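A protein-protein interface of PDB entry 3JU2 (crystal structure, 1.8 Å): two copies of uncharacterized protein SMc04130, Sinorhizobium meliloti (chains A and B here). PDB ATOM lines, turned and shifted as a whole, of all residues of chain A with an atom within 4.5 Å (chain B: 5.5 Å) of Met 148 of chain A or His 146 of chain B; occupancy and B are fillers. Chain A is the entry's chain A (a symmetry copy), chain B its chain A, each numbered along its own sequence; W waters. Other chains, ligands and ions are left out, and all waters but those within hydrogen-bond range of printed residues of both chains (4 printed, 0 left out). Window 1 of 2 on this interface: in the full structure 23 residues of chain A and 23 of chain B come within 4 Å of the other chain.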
ATOM      1  N   HIS A 146     -25.876 -18.086  25.083  1.00  0.00           N
ATOM      2  CA  HIS A 146     -24.434 -18.054  25.209  1.00  0.00           C
ATOM      3  C   HIS A 146     -23.844 -19.478  25.367  1.00  0.00           C
ATOM      4  O   HIS A 146     -24.390 -20.305  26.116  1.00  0.00           O
ATOM      5  CB  HIS A 146     -24.023 -17.215  26.425  1.00  0.00           C
ATOM      6  CG  HIS A 146     -22.608 -16.758  26.357  1.00  0.00           C
ATOM      7  ND1 HIS A 146     -21.541 -17.609  26.548  1.00  0.00           N
ATOM      8  CD2 HIS A 146     -22.078 -15.543  26.067  1.00  0.00           C
ATOM      9  CE1 HIS A 146     -20.413 -16.933  26.398  1.00  0.00           C
ATOM     10  NE2 HIS A 146     -20.713 -15.673  26.128  1.00  0.00           N
ATOM     11  N   PRO A 147     -22.754 -19.766  24.637  1.00  0.00           N
ATOM     12  CA  PRO A 147     -22.011 -21.040  24.775  1.00  0.00           C
ATOM     13  C   PRO A 147     -21.744 -21.501  26.225  1.00  0.00           C
ATOM     14  O   PRO A 147     -21.724 -22.681  26.469  1.00  0.00           O
ATOM     15  CB  PRO A 147     -20.707 -20.747  24.060  1.00  0.00           C
ATOM     16  CG  PRO A 147     -21.164 -19.896  22.932  1.00  0.00           C
ATOM     17  CD  PRO A 147     -22.194 -18.948  23.556  1.00  0.00           C
ATOM     18  N   MET A 148     -21.591 -20.580  27.178  1.00  0.00           N
ATOM     19  CA  MET A 148     -21.382 -21.005  28.580  1.00  0.00           C
ATOM     20  C   MET A 148     -22.564 -21.764  29.183  1.00  0.00           C
ATOM     21  O   MET A 148     -22.410 -22.469  30.200  1.00  0.00           O
ATOM     22  CB  MET A 148     -20.906 -19.836  29.481  1.00  0.00           C
ATOM     23  CG  MET A 148     -21.912 -18.765  29.875  1.00  0.00           C
ATOM     24  SD  MET A 148     -21.030 -17.332  30.682  1.00  0.00           S
ATOM     25  CE  MET A 148     -22.292 -16.109  30.354  1.00  0.00           C
ATOM     26  N   TYR A 149     -23.730 -21.651  28.549  1.00  0.00           N
ATOM     27  CA  TYR A 149     -24.947 -22.309  29.016  1.00  0.00           C
ATOM     28  C   TYR A 149     -25.262 -23.666  28.371  1.00  0.00           C
ATOM     29  O   TYR A 149     -26.335 -24.225  28.610  1.00  0.00           O
ATOM     30  CB  TYR A 149     -26.145 -21.387  28.820  1.00  0.00           C
ATOM     31  CG  TYR A 149     -26.019 -20.053  29.504  1.00  0.00           C
ATOM     32  CD1 TYR A 149     -25.713 -19.955  30.878  1.00  0.00           C
ATOM     33  CD2 TYR A 149     -26.213 -18.880  28.789  1.00  0.00           C
ATOM     34  CE1 TYR A 149     -25.614 -18.699  31.496  1.00  0.00           C
ATOM     35  CE2 TYR A 149     -26.122 -17.634  29.384  1.00  0.00           C
ATOM     36  CZ  TYR A 149     -25.816 -17.534  30.730  1.00  0.00           C
ATOM     37  OH  TYR A 149     -25.731 -16.257  31.254  1.00  0.00           O
ATOM     38  N   ALA A 150     -24.336 -24.156  27.560  1.00  0.00           N
ATOM     39  CA  ALA A 150     -24.568 -25.315  26.672  1.00  0.00           C
ATOM     40  C   ALA A 150     -24.899 -26.614  27.408  1.00  0.00           C
ATOM     41  O   ALA A 150     -25.814 -27.343  27.002  1.00  0.00           O
ATOM     42  CB  ALA A 150     -23.368 -25.517  25.731  1.00  0.00           C
ATOM     43  N   TYR A 180     -26.691 -10.513  24.651  1.00  0.00           N
ATOM     44  CA  TYR A 180     -25.880 -11.172  25.683  1.00  0.00           C
ATOM     45  C   TYR A 180     -25.375 -12.515  25.158  1.00  0.00           C
ATOM     46  O   TYR A 180     -24.226 -12.883  25.381  1.00  0.00           O
ATOM     47  CB  TYR A 180     -26.679 -11.399  26.968  1.00  0.00           C
ATOM     48  CG  TYR A 180     -25.792 -11.550  28.180  1.00  0.00           C
ATOM     49  CD1 TYR A 180     -25.138 -10.442  28.712  1.00  0.00           C
ATOM     50  CD2 TYR A 180     -25.605 -12.801  28.793  1.00  0.00           C
ATOM     51  CE1 TYR A 180     -24.297 -10.567  29.830  1.00  0.00           C
ATOM     52  CE2 TYR A 180     -24.783 -12.941  29.935  1.00  0.00           C
ATOM     53  CZ  TYR A 180     -24.142 -11.811  30.447  1.00  0.00           C
ATOM     54  OH  TYR A 180     -23.331 -11.921  31.547  1.00  0.00           O
ATOM     55  N   TRP A 209     -22.687  -6.726  28.217  1.00  0.00           N
ATOM     56  CA  TRP A 209     -21.687  -7.659  28.711  1.00  0.00           C
ATOM     57  C   TRP A 209     -20.684  -6.855  29.532  1.00  0.00           C
ATOM     58  O   TRP A 209     -19.891  -6.060  29.003  1.00  0.00           O
ATOM     59  CB  TRP A 209     -20.960  -8.367  27.544  1.00  0.00           C
ATOM     60  CG  TRP A 209     -19.993  -9.405  28.021  1.00  0.00           C
ATOM     61  CD1 TRP A 209     -18.686  -9.216  28.360  1.00  0.00           C
ATOM     62  CD2 TRP A 209     -20.278 -10.792  28.264  1.00  0.00           C
ATOM     63  NE1 TRP A 209     -18.135 -10.401  28.790  1.00  0.00           N
ATOM     64  CE2 TRP A 209     -19.085 -11.383  28.739  1.00  0.00           C
ATOM     65  CE3 TRP A 209     -21.426 -11.586  28.130  1.00  0.00           C
ATOM     66  CZ2 TRP A 209     -18.990 -12.758  29.076  1.00  0.00           C
ATOM     67  CZ3 TRP A 209     -21.341 -12.955  28.457  1.00  0.00           C
ATOM     68  CH2 TRP A 209     -20.129 -13.517  28.939  1.00  0.00           C
ATOM     69  N   MET A 216     -21.903 -16.157  36.111  1.00  0.00           N
ATOM     70  CA  MET A 216     -22.280 -16.689  34.800  1.00  0.00           C
ATOM     71  C   MET A 216     -23.736 -16.458  34.384  1.00  0.00           C
ATOM     72  O   MET A 216     -24.038 -16.473  33.188  1.00  0.00           O
ATOM     73  CB  MET A 216     -21.877 -18.168  34.674  1.00  0.00           C
ATOM     74  CG  MET A 216     -20.339 -18.311  34.783  1.00  0.00           C
ATOM     75  SD  MET A 216     -19.845 -20.019  34.930  1.00  0.00           S
ATOM     76  CE  MET A 216     -20.266 -20.626  33.279  1.00  0.00           C
ATOM     77  N   PRO B 144      -8.198 -21.082  20.057  1.00  0.00           N
ATOM     78  CA  PRO B 144      -9.468 -20.413  20.231  1.00  0.00           C
ATOM     79  C   PRO B 144      -9.933 -20.559  21.686  1.00  0.00           C
ATOM     80  O   PRO B 144      -9.805 -21.644  22.269  1.00  0.00           O
ATOM     81  CB  PRO B 144     -10.406 -21.171  19.294  1.00  0.00           C
ATOM     82  CG  PRO B 144      -9.764 -22.478  19.033  1.00  0.00           C
ATOM     83  CD  PRO B 144      -8.301 -22.224  19.114  1.00  0.00           C
ATOM     84  N   LEU B 145     -10.390 -19.457  22.268  1.00  0.00           N
ATOM     85  CA  LEU B 145     -10.864 -19.458  23.657  1.00  0.00           C
ATOM     86  C   LEU B 145     -12.365 -19.458  23.730  1.00  0.00           C
ATOM     87  O   LEU B 145     -13.062 -18.930  22.849  1.00  0.00           O
ATOM     88  CB  LEU B 145     -10.294 -18.276  24.449  1.00  0.00           C
ATOM     89  CG  LEU B 145      -9.179 -18.632  25.443  1.00  0.00           C
ATOM     90  CD1 LEU B 145      -7.917 -19.161  24.781  1.00  0.00           C
ATOM     91  CD2 LEU B 145      -8.837 -17.407  26.333  1.00  0.00           C
ATOM     92  N   HIS B 146     -12.883 -20.068  24.787  1.00  0.00           N
ATOM     93  CA  HIS B 146     -14.306 -20.041  25.046  1.00  0.00           C
ATOM     94  C   HIS B 146     -14.899 -18.627  24.825  1.00  0.00           C
ATOM     95  O   HIS B 146     -14.300 -17.622  25.242  1.00  0.00           O
ATOM     96  CB  HIS B 146     -14.596 -20.475  26.488  1.00  0.00           C
ATOM     97  CG  HIS B 146     -16.004 -20.912  26.686  1.00  0.00           C
ATOM     98  ND1 HIS B 146     -17.062 -20.028  26.711  1.00  0.00           N
ATOM     99  CD2 HIS B 146     -16.542 -22.151  26.821  1.00  0.00           C
ATOM    100  CE1 HIS B 146     -18.189 -20.702  26.870  1.00  0.00           C
ATOM    101  NE2 HIS B 146     -17.897 -21.990  26.961  1.00  0.00           N
ATOM    102  N   PRO B 147     -16.055 -18.554  24.143  1.00  0.00           N
ATOM    103  CA  PRO B 147     -16.800 -17.287  23.962  1.00  0.00           C
ATOM    104  C   PRO B 147     -16.942 -16.412  25.228  1.00  0.00           C
ATOM    105  O   PRO B 147     -16.956 -15.212  25.110  1.00  0.00           O
ATOM    106  CB  PRO B 147     -18.159 -17.762  23.487  1.00  0.00           C
ATOM    107  CG  PRO B 147     -17.793 -18.916  22.627  1.00  0.00           C
ATOM    108  CD  PRO B 147     -16.698 -19.649  23.410  1.00  0.00           C
ATOM    109  N   MET B 148     -16.996 -17.005  26.421  1.00  0.00           N
ATOM    110  CA  MET B 148     -17.084 -16.179  27.646  1.00  0.00           C
ATOM    111  C   MET B 148     -15.863 -15.291  27.887  1.00  0.00           C
ATOM    112  O   MET B 148     -15.935 -14.313  28.658  1.00  0.00           O
ATOM    113  CB  MET B 148     -17.461 -17.021  28.893  1.00  0.00           C
ATOM    114  CG  MET B 148     -16.409 -17.940  29.496  1.00  0.00           C
ATOM    115  SD  MET B 148     -17.195 -19.056  30.768  1.00  0.00           S
ATOM    116  CE  MET B 148     -15.951 -20.338  30.708  1.00  0.00           C
ATOM    117  N   TYR B 149     -14.757 -15.604  27.214  1.00  0.00           N
ATOM    118  CA  TYR B 149     -13.512 -14.853  27.352  1.00  0.00           C
ATOM    119  C   TYR B 149     -13.276 -13.754  26.308  1.00  0.00           C
ATOM    120  O   TYR B 149     -12.193 -13.165  26.271  1.00  0.00           O
ATOM    121  CB  TYR B 149     -12.324 -15.809  27.333  1.00  0.00           C
ATOM    122  CG  TYR B 149     -12.370 -16.877  28.392  1.00  0.00           C
ATOM    123  CD1 TYR B 149     -12.551 -16.558  29.754  1.00  0.00           C
ATOM    124  CD2 TYR B 149     -12.225 -18.212  28.043  1.00  0.00           C
ATOM    125  CE1 TYR B 149     -12.576 -17.572  30.724  1.00  0.00           C
ATOM    126  CE2 TYR B 149     -12.245 -19.223  28.987  1.00  0.00           C
ATOM    127  CZ  TYR B 149     -12.428 -18.913  30.324  1.00  0.00           C
ATOM    128  OH  TYR B 149     -12.448 -19.976  31.210  1.00  0.00           O
ATOM    129  N   ALA B 150     -14.277 -13.515  25.474  1.00  0.00           N
ATOM    130  CA  ALA B 150     -14.142 -12.676  24.264  1.00  0.00           C
ATOM    131  C   ALA B 150     -13.764 -11.221  24.548  1.00  0.00           C
ATOM    132  O   ALA B 150     -12.899 -10.660  23.863  1.00  0.00           O
ATOM    133  CB  ALA B 150     -15.424 -12.747  23.418  1.00  0.00           C
ATOM    134  N   ALA B 154      -9.413 -13.089  25.075  1.00  0.00           N
ATOM    135  CA  ALA B 154      -9.120 -13.524  23.689  1.00  0.00           C
ATOM    136  C   ALA B 154     -10.358 -13.416  22.824  1.00  0.00           C
ATOM    137  O   ALA B 154     -11.398 -13.966  23.159  1.00  0.00           O
ATOM    138  CB  ALA B 154      -8.564 -14.952  23.637  1.00  0.00           C
ATOM    139  N   ASN B 157     -12.497 -16.923  19.178  1.00  0.00           N
ATOM    140  CA  ASN B 157     -13.470 -17.653  20.005  1.00  0.00           C
ATOM    141  C   ASN B 157     -14.104 -18.873  19.385  1.00  0.00           C
ATOM    142  O   ASN B 157     -14.947 -19.493  20.023  1.00  0.00           O
ATOM    143  CB  ASN B 157     -14.590 -16.708  20.472  1.00  0.00           C
ATOM    144  CG  ASN B 157     -14.030 -15.517  21.219  1.00  0.00           C
ATOM    145  OD1 ASN B 157     -14.079 -14.389  20.737  1.00  0.00           O
ATOM    146  ND2 ASN B 157     -13.421 -15.778  22.363  1.00  0.00           N
ATOM    147  N   TYR B 180     -12.006 -27.437  26.557  1.00  0.00           N
ATOM    148  CA  TYR B 180     -12.731 -26.490  27.414  1.00  0.00           C
ATOM    149  C   TYR B 180     -13.299 -25.358  26.561  1.00  0.00           C
ATOM    150  O   TYR B 180     -14.428 -24.924  26.767  1.00  0.00           O
ATOM    151  CB  TYR B 180     -11.822 -25.902  28.496  1.00  0.00           C
ATOM    152  CG  TYR B 180     -12.598 -25.384  29.683  1.00  0.00           C
ATOM    153  CD1 TYR B 180     -13.187 -26.276  30.577  1.00  0.00           C
ATOM    154  CD2 TYR B 180     -12.748 -24.006  29.910  1.00  0.00           C
ATOM    155  CE1 TYR B 180     -13.926 -25.812  31.678  1.00  0.00           C
ATOM    156  CE2 TYR B 180     -13.465 -23.521  31.027  1.00  0.00           C
ATOM    157  CZ  TYR B 180     -14.041 -24.438  31.907  1.00  0.00           C
ATOM    158  OH  TYR B 180     -14.753 -23.995  32.994  1.00  0.00           O
ATOM    159  N   HIS B 181     -12.503 -24.932  25.593  1.00  0.00           N
ATOM    160  CA  HIS B 181     -12.857 -23.811  24.736  1.00  0.00           C
ATOM    161  C   HIS B 181     -13.820 -24.132  23.588  1.00  0.00           C
ATOM    162  O   HIS B 181     -14.555 -23.254  23.152  1.00  0.00           O
ATOM    163  CB  HIS B 181     -11.571 -23.177  24.228  1.00  0.00           C
ATOM    164  CG  HIS B 181     -10.688 -22.669  25.326  1.00  0.00           C
ATOM    165  ND1 HIS B 181     -11.186 -22.035  26.450  1.00  0.00           N
ATOM    166  CD2 HIS B 181      -9.343 -22.683  25.463  1.00  0.00           C
ATOM    167  CE1 HIS B 181     -10.177 -21.689  27.234  1.00  0.00           C
ATOM    168  NE2 HIS B 181      -9.052 -22.073  26.657  1.00  0.00           N
ATOM    169  N   TRP B 183     -15.668 -27.533  23.070  1.00  0.00           N
ATOM    170  CA  TRP B 183     -16.563 -28.709  23.170  1.00  0.00           C
ATOM    171  C   TRP B 183     -18.022 -28.419  22.780  1.00  0.00           C
ATOM    172  O   TRP B 183     -18.692 -29.284  22.235  1.00  0.00           O
ATOM    173  CB  TRP B 183     -16.516 -29.353  24.592  1.00  0.00           C
ATOM    174  CG  TRP B 183     -17.299 -28.549  25.594  1.00  0.00           C
ATOM    175  CD1 TRP B 183     -16.873 -27.444  26.293  1.00  0.00           C
ATOM    176  CD2 TRP B 183     -18.666 -28.743  25.942  1.00  0.00           C
ATOM    177  NE1 TRP B 183     -17.900 -26.956  27.067  1.00  0.00           N
ATOM    178  CE2 TRP B 183     -19.014 -27.729  26.863  1.00  0.00           C
ATOM    179  CE3 TRP B 183     -19.637 -29.686  25.567  1.00  0.00           C
ATOM    180  CZ2 TRP B 183     -20.288 -27.623  27.403  1.00  0.00           C
ATOM    181  CZ3 TRP B 183     -20.896 -29.596  26.112  1.00  0.00           C
ATOM    182  CH2 TRP B 183     -21.222 -28.558  27.019  1.00  0.00           C
ATOM    183  N   TRP B 184     -18.510 -27.207  23.098  1.00  0.00           N
ATOM    184  CA  TRP B 184     -19.901 -26.784  22.914  1.00  0.00           C
ATOM    185  C   TRP B 184     -20.242 -26.501  21.420  1.00  0.00           C
ATOM    186  O   TRP B 184     -21.422 -26.353  21.053  1.00  0.00           O
ATOM    187  CB  TRP B 184     -20.131 -25.500  23.759  1.00  0.00           C
ATOM    188  CG  TRP B 184     -19.199 -24.448  23.304  1.00  0.00           C
ATOM    189  CD1 TRP B 184     -17.920 -24.220  23.720  1.00  0.00           C
ATOM    190  CD2 TRP B 184     -19.429 -23.562  22.211  1.00  0.00           C
ATOM    191  NE1 TRP B 184     -17.345 -23.219  22.969  1.00  0.00           N
ATOM    192  CE2 TRP B 184     -18.258 -22.793  22.040  1.00  0.00           C
ATOM    193  CE3 TRP B 184     -20.538 -23.317  21.378  1.00  0.00           C
ATOM    194  CZ2 TRP B 184     -18.146 -21.829  21.038  1.00  0.00           C
ATOM    195  CZ3 TRP B 184     -20.427 -22.359  20.394  1.00  0.00           C
ATOM    196  CH2 TRP B 184     -19.247 -21.611  20.244  1.00  0.00           C
ATOM    197  N   TRP B 209     -15.621 -29.936  31.432  1.00  0.00           N
ATOM    198  CA  TRP B 209     -16.586 -28.885  31.714  1.00  0.00           C
ATOM    199  C   TRP B 209     -17.501 -29.395  32.824  1.00  0.00           C
ATOM    200  O   TRP B 209     -18.326 -30.300  32.628  1.00  0.00           O
ATOM    201  CB  TRP B 209     -17.425 -28.546  30.459  1.00  0.00           C
ATOM    202  CG  TRP B 209     -18.359 -27.400  30.691  1.00  0.00           C
ATOM    203  CD1 TRP B 209     -19.627 -27.462  31.187  1.00  0.00           C
ATOM    204  CD2 TRP B 209     -18.072 -26.008  30.483  1.00  0.00           C
ATOM    205  NE1 TRP B 209     -20.154 -26.196  31.293  1.00  0.00           N
ATOM    206  CE2 TRP B 209     -19.225 -25.286  30.866  1.00  0.00           C
ATOM    207  CE3 TRP B 209     -16.952 -25.306  30.017  1.00  0.00           C
ATOM    208  CZ2 TRP B 209     -19.308 -23.872  30.786  1.00  0.00           C
ATOM    209  CZ3 TRP B 209     -17.026 -23.900  29.928  1.00  0.00           C
ATOM    210  CH2 TRP B 209     -18.197 -23.203  30.328  1.00  0.00           C
ATOM    211  N   MET B 216     -15.822 -18.573  36.200  1.00  0.00           N
ATOM    212  CA  MET B 216     -15.572 -18.461  34.761  1.00  0.00           C
ATOM    213  C   MET B 216     -14.156 -18.826  34.304  1.00  0.00           C
ATOM    214  O   MET B 216     -13.963 -19.171  33.136  1.00  0.00           O
ATOM    215  CB  MET B 216     -16.006 -17.081  34.238  1.00  0.00           C
ATOM    216  CG  MET B 216     -17.529 -16.892  34.436  1.00  0.00           C
ATOM    217  SD  MET B 216     -18.031 -15.210  34.113  1.00  0.00           S
ATOM    218  CE  MET B 216     -17.768 -15.128  32.326  1.00  0.00           C
HETATM  219  O   HOH W   1     -19.022 -13.476  25.809  1.00  0.00           O
HETATM  220  O   HOH W   2     -15.257 -11.721  28.292  1.00  0.00           O
HETATM  221  O   HOH W   3     -23.082 -25.044  30.684  1.00  0.00           O
HETATM  222  O   HOH W   4     -19.580 -24.159  27.464  1.00  0.00           O
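The backbone NH (N) of Met 148 of chain B lies within hydrogen-bond range of a ring nitrogen (ND1) of His 146 of chain B, 3.0 Å away.
The backbone NH of His 146 of chain B lies within hydrogen-bond range of a ring nitrogen (ND1) of His 181 of chain B (3.1 Å).
The side-chain hydroxyl (OH) of Tyr 149 of chain B sits at hydrogen-bond distance from the backbone carbonyl oxygen (O) of Met 216 of chain B (2.6 Å).
O of His 181 of chain B sits at hydrogen-bond distance from NE1 of Trp 184 of chain B, at 2.8 Å.
A ring nitrogen (ND1) of His 146 of chain A is in hydrogen-bond range of the backbone NH (N) of Met 148 of chain A (3.0 Å).
The side-chain hydroxyl of Tyr 149 of chain A lies within hydrogen-bond range of the backbone carbonyl oxygen of Met 216 of chain A (2.6 Å).
Among the printed residues, pairs that only touch across the chains: Met 216 of chain A with Met 216 of chain B (3.2 Å), His 146 of chain A with Met 148 of chain B (3.4 Å), Met 148 of chain A with His 146 of chain B (3.4 Å), Trp 209 of chain A with Met 148 of chain B (3.5 Å), Met 148 of chain A with Trp 209 of chain B (3.5 Å), Pro 147 of chain A with Pro 147 of chain B (3.5 Å), Pro 147 of chain A with Trp 184 of chain B (3.6 Å), His 146 of chain A with Pro 147 of chain B (3.7 Å), Pro 147 of chain A with His 146 of chain B (3.7 Å), Ala 150 of chain A with Trp 184 of chain B (3.8 Å) and Ala 150 of chain A with Trp 183 of chain B (3.9 Å).
Of the printed residues of chain B, Met 148 of chain A touches His 146 and Trp 209.
Of chain A, only Pro 147 and Met 148 come within 4 Å of His 146 of chain B.
Printed residues of chain A within 4 Å of Met 216 of chain B: Met 216.
Printed residues of chain B within 4 Å of Met 216 of chain A: Met 216 (3.2 Å).
Pro 144 of chain B touches none of the printed residues of chain A.
Asn 157 of chain B touches none of the printed residues of chain A.
The nearest printed residue of chain B that does not touch Met 148 of chain A is Met 148 of chain B (4.004 Å).
The nearest residue of chain A that does not touch His 146 of chain B is His 146 of chain A (4.4 Å).
The nearest printed residue of chain B that does not touch Pro 147 of chain A is Trp 209 of chain B (5.1 Å).
Of the 8 printed residues of chain A, 6 touch a printed residue of chain B.
Among the printed residues, no Asp or Glu carboxylate lies within 4 Å of a Lys or Arg side-chain nitrogen of the other chain.
His 146 of chain A touches Pro 147 of chain B, and with the chains exchanged Pro 147 of chain A touches His 146 of chain B.
His 146 of chain A touches Met 148 of chain B, and with the chains exchanged Met 148 of chain A touches His 146 of chain B.
Met 148 of chain A touches Trp 209 of chain B, and with the chains exchanged Trp 209 of chain A touches Met 148 of chain B.
Met 216 of chain A touches its own counterpart, Met 216 of chain B.
Of the 11 pairs that touch across the chains among the printed residues, 8 have their exchanged pair printed and touching as well.
Water W2 lies within hydrogen-bond range of the backbone carbonyl oxygen (O) of Met 148 of chain B, the indole nitrogen (NE1) of Trp 209 of chain A and the backbone NH (N) of Ala 150 of chain B.
Water W3 lies within hydrogen-bond range of O of Met 148 of chain A (2.7 Å), NE1 of Trp 209 of chain B (3.2 Å) and N of Ala 150 of chain A (3.5 Å).
Water W1 bridges O of Pro 147 of chain B and NE2 of His 146 of chain A.
Water W4 lies within hydrogen-bond range of the backbone carbonyl oxygen (O) of Pro 147 of chain A (2.8 Å), a ring nitrogen (NE2) of His 146 of chain B (2.8 Å) and the indole nitrogen (NE1) of Trp 183 of chain B (3.3 Å).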
